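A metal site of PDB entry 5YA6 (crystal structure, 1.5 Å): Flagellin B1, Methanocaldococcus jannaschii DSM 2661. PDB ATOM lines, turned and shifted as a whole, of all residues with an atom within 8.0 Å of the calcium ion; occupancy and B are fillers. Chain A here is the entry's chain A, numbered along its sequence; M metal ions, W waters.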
ATOM      1  N   PRO A  38      24.505 -24.171   8.791  1.00  0.00           N
ATOM      2  CA  PRO A  38      24.931 -22.774   8.712  1.00  0.00           C
ATOM      3  C   PRO A  38      25.952 -22.361   9.752  1.00  0.00           C
ATOM      4  O   PRO A  38      25.957 -22.887  10.853  1.00  0.00           O
ATOM      5  CB  PRO A  38      23.624 -22.025   8.850  1.00  0.00           C
ATOM      6  CG  PRO A  38      22.546 -23.012   8.519  1.00  0.00           C
ATOM      7  CD  PRO A  38      23.054 -24.291   9.105  1.00  0.00           C
ATOM      8  N   PRO A  44      18.975 -16.991   7.108  1.00  0.00           N
ATOM      9  CA  PRO A  44      18.596 -18.122   6.260  1.00  0.00           C
ATOM     10  C   PRO A  44      19.246 -18.088   4.893  1.00  0.00           C
ATOM     11  O   PRO A  44      19.421 -16.999   4.321  1.00  0.00           O
ATOM     12  CB  PRO A  44      17.071 -18.002   6.173  1.00  0.00           C
ATOM     13  CG  PRO A  44      16.708 -17.202   7.405  1.00  0.00           C
ATOM     14  CD  PRO A  44      17.799 -16.207   7.513  1.00  0.00           C
ATOM     15  N   VAL A  99      17.144 -33.940   4.206  1.00  0.00           N
ATOM     16  CA  VAL A  99      16.989 -33.288   5.481  1.00  0.00           C
ATOM     17  C   VAL A  99      17.498 -34.243   6.557  1.00  0.00           C
ATOM     18  O   VAL A  99      17.180 -35.455   6.559  1.00  0.00           O
ATOM     19  CB  VAL A  99      15.507 -33.069   5.748  1.00  0.00           C
ATOM     20  CG1 VAL A  99      15.332 -32.401   7.088  1.00  0.00           C
ATOM     21  CG2 VAL A  99      14.858 -32.264   4.581  1.00  0.00           C
ATOM     22  N   GLN A 101      18.393 -32.585  10.034  1.00  0.00           N
ATOM     23  CA  GLN A 101      17.803 -31.923  11.199  1.00  0.00           C
ATOM     24  C   GLN A 101      17.107 -30.626  10.745  1.00  0.00           C
ATOM     25  O   GLN A 101      17.692 -29.721  10.082  1.00  0.00           O
ATOM     26  CB  GLN A 101      18.854 -31.589  12.277  1.00  0.00           C
ATOM     27  CG  GLN A 101      18.239 -31.105  13.584  1.00  0.00           C
ATOM     28  CD  GLN A 101      19.243 -31.050  14.683  1.00  0.00           C
ATOM     29  OE1 GLN A 101      19.864 -30.006  14.928  1.00  0.00           O
ATOM     30  NE2 GLN A 101      19.418 -32.163  15.354  1.00  0.00           N
ATOM     31  N   ASP A 102      15.826 -30.474  11.163  1.00  0.00           N
ATOM     32  CA  ASP A 102      15.063 -29.299  10.730  1.00  0.00           C
ATOM     33  C   ASP A 102      13.993 -29.139  11.850  1.00  0.00           C
ATOM     34  O   ASP A 102      13.615 -30.139  12.501  1.00  0.00           O
ATOM     35  CB  ASP A 102      14.433 -29.511   9.373  1.00  0.00           C
ATOM     36  CG  ASP A 102      13.920 -28.192   8.701  1.00  0.00           C
ATOM     37  OD1 ASP A 102      14.035 -27.112   9.355  1.00  0.00           O
ATOM     38  OD2 ASP A 102      13.580 -28.270   7.484  1.00  0.00           O
ATOM     39  N   ALA A 103      13.606 -27.903  12.124  1.00  0.00           N
ATOM     40  CA  ALA A 103      12.542 -27.641  13.147  1.00  0.00           C
ATOM     41  C   ALA A 103      11.444 -26.705  12.650  1.00  0.00           C
ATOM     42  O   ALA A 103      10.548 -26.417  13.407  1.00  0.00           O
ATOM     43  CB  ALA A 103      13.167 -27.042  14.389  1.00  0.00           C
ATOM     44  N   ASP A 104      11.526 -26.210  11.443  1.00  0.00           N
ATOM     45  CA  ASP A 104      10.527 -25.309  10.866  1.00  0.00           C
ATOM     46  C   ASP A 104      10.072 -25.649   9.453  1.00  0.00           C
ATOM     47  O   ASP A 104       9.367 -24.873   8.790  1.00  0.00           O
ATOM     48  CB  ASP A 104      10.948 -23.856  11.007  1.00  0.00           C
ATOM     49  CG  ASP A 104      12.109 -23.468  10.126  1.00  0.00           C
ATOM     50  OD1 ASP A 104      12.705 -24.319   9.415  1.00  0.00           O
ATOM     51  OD2 ASP A 104      12.339 -22.238  10.071  1.00  0.00           O
ATOM     52  N   GLY A 105      10.504 -26.775   8.908  1.00  0.00           N
ATOM     53  CA  GLY A 105      10.163 -27.200   7.581  1.00  0.00           C
ATOM     54  C   GLY A 105      10.920 -26.447   6.438  1.00  0.00           C
ATOM     55  O   GLY A 105      10.695 -26.715   5.269  1.00  0.00           O
ATOM     56  N   SER A 106      11.848 -25.569   6.836  1.00  0.00           N
ATOM     57  CA  SER A 106      12.519 -24.761   5.826  1.00  0.00           C
ATOM     58  C   SER A 106      13.269 -25.551   4.782  1.00  0.00           C
ATOM     59  O   SER A 106      13.217 -25.200   3.591  1.00  0.00           O
ATOM     60  CB  SER A 106      13.461 -23.746   6.462  1.00  0.00           C
ATOM     61  OG  SER A 106      14.557 -24.338   7.134  1.00  0.00           O
ATOM     62  N   LEU A 107      13.924 -26.641   5.174  1.00  0.00           N
ATOM     63  CA  LEU A 107      14.646 -27.409   4.223  1.00  0.00           C
ATOM     64  C   LEU A 107      13.742 -28.125   3.237  1.00  0.00           C
ATOM     65  O   LEU A 107      14.138 -28.369   2.108  1.00  0.00           O
ATOM     66  CB  LEU A 107      15.538 -28.401   4.929  1.00  0.00           C
ATOM     67  CG  LEU A 107      16.874 -27.924   5.449  1.00  0.00           C
ATOM     68  CD1 LEU A 107      17.602 -28.955   6.308  1.00  0.00           C
ATOM     69  CD2 LEU A 107      17.724 -27.520   4.224  1.00  0.00           C
ATOM     70  N   SER A 108      12.479 -28.325   3.605  1.00  0.00           N
ATOM     71  CA  SER A 108      11.535 -28.950   2.650  1.00  0.00           C
ATOM     72  C   SER A 108      11.299 -28.077   1.450  1.00  0.00           C
ATOM     73  O   SER A 108      10.865 -28.577   0.402  1.00  0.00           O
ATOM     74  CB  SER A 108      10.233 -29.350   3.342  1.00  0.00           C
ATOM     75  OG  SER A 108      10.508 -30.377   4.301  1.00  0.00           O
ATOM     76  N   VAL A 111      15.526 -24.156   1.973  1.00  0.00           N
ATOM     77  CA  VAL A 111      16.088 -23.082   2.740  1.00  0.00           C
ATOM     78  C   VAL A 111      16.685 -23.682   4.013  1.00  0.00           C
ATOM     79  O   VAL A 111      15.994 -24.368   4.753  1.00  0.00           O
ATOM     80  CB  VAL A 111      15.054 -21.982   3.079  1.00  0.00           C
ATOM     81  CG1 VAL A 111      15.651 -20.935   3.991  1.00  0.00           C
ATOM     82  CG2 VAL A 111      14.501 -21.348   1.799  1.00  0.00           C
ATOM     83  N   ILE A 112      17.946 -23.380   4.284  1.00  0.00           N
ATOM     84  CA  ILE A 112      18.654 -23.864   5.478  1.00  0.00           C
ATOM     85  C   ILE A 112      18.788 -22.722   6.443  1.00  0.00           C
ATOM     86  O   ILE A 112      19.228 -21.628   6.066  1.00  0.00           O
ATOM     87  CB  ILE A 112      19.979 -24.555   5.074  1.00  0.00           C
ATOM     88  CG1 ILE A 112      20.507 -25.353   6.257  1.00  0.00           C
ATOM     89  CG2 ILE A 112      21.010 -23.577   4.505  1.00  0.00           C
ATOM     90  CD1 ILE A 112      21.674 -26.276   5.883  1.00  0.00           C
ATOM     91  N   ASN A 113      18.396 -22.940   7.717  1.00  0.00           N
ATOM     92  CA  ASN A 113      18.502 -21.860   8.710  1.00  0.00           C
ATOM     93  C   ASN A 113      18.991 -22.405   9.992  1.00  0.00           C
ATOM     94  O   ASN A 113      19.407 -23.558  10.060  1.00  0.00           O
ATOM     95  CB  ASN A 113      17.185 -21.010   8.789  1.00  0.00           C
ATOM     96  CG  ASN A 113      15.967 -21.818   9.177  1.00  0.00           C
ATOM     97  OD1 ASN A 113      16.098 -22.916   9.628  1.00  0.00           O
ATOM     98  ND2 ASN A 113      14.742 -21.283   8.898  1.00  0.00           N
ATOM     99  N   LYS A 114      18.949 -21.604  11.051  1.00  0.00           N
ATOM    100  CA  LYS A 114      19.704 -21.861  12.279  1.00  0.00           C
ATOM    101  C   LYS A 114      19.335 -23.209  12.878  1.00  0.00           C
ATOM    102  O   LYS A 114      18.131 -23.549  13.029  1.00  0.00           O
ATOM    103  CB  LYS A 114      19.393 -20.779  13.309  1.00  0.00           C
ATOM    104  CG  LYS A 114      20.059 -20.924  14.655  1.00  0.00           C
ATOM    105  CD  LYS A 114      19.403 -19.971  15.656  1.00  0.00           C
ATOM    106  CE  LYS A 114      19.875 -20.170  17.064  1.00  0.00           C
ATOM    107  NZ  LYS A 114      19.461 -21.450  17.653  1.00  0.00           N
ATOM    108  N   GLY A 115      20.369 -24.001  13.096  1.00  0.00           N
ATOM    109  CA  GLY A 115      20.265 -25.300  13.740  1.00  0.00           C
ATOM    110  C   GLY A 115      20.070 -26.479  12.765  1.00  0.00           C
ATOM    111  O   GLY A 115      20.213 -27.632  13.180  1.00  0.00           O
ATOM    112  N   ASP A 116      19.779 -26.192  11.507  1.00  0.00           N
ATOM    113  CA  ASP A 116      19.502 -27.219  10.504  1.00  0.00           C
ATOM    114  C   ASP A 116      20.773 -27.981  10.122  1.00  0.00           C
ATOM    115  O   ASP A 116      21.884 -27.370  10.082  1.00  0.00           O
ATOM    116  CB  ASP A 116      19.003 -26.603   9.213  1.00  0.00           C
ATOM    117  CG  ASP A 116      17.510 -26.055   9.312  1.00  0.00           C
ATOM    118  OD1 ASP A 116      16.850 -26.212  10.362  1.00  0.00           O
ATOM    119  OD2 ASP A 116      17.088 -25.513   8.264  1.00  0.00           O
ATOM    120  N   ILE A 117      20.623 -29.249   9.824  1.00  0.00           N
ATOM    121  CA  ILE A 117      21.662 -29.989   9.112  1.00  0.00           C
ATOM    122  C   ILE A 117      21.059 -30.620   7.895  1.00  0.00           C
ATOM    123  O   ILE A 117      19.928 -31.166   7.914  1.00  0.00           O
ATOM    124  CB  ILE A 117      22.237 -31.107  10.011  1.00  0.00           C
ATOM    125  CG1 ILE A 117      22.809 -30.511  11.291  1.00  0.00           C
ATOM    126  CG2 ILE A 117      23.260 -31.972   9.195  1.00  0.00           C
ATOM    127  CD1 ILE A 117      23.216 -31.586  12.332  1.00  0.00           C
HETATM  128 CA    CA M   1      14.964 -24.979   9.421  1.00  0.00          CA
HETATM  129  O   HOH W   1      14.590 -24.950  11.829  1.00  0.00           O
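OD2 of Asp 102 sits at hydrogen-bond distance from N of Leu 107 (2.8 Å). N of Val 111 is in hydrogen-bond range of O of Ser 106, at 3.0 Å.
Five residues have an atom within 4 Å of the calcium ion: Asp 102, Asp 104, Ser 106, Asn 113 and Asp 116.
The calcium ion is bound by the side-chain carboxylate (OD1) of Asp 102, the side-chain carboxylate (OD1) of Asp 104, the side-chain amide oxygen (OD1) of Asn 113, the side-chain hydroxyl (OG) of Ser 106, water W1, the side-chain carboxylate (OD1) of Asp 116 and the side-chain carboxylate (OD2) of Asp 116.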
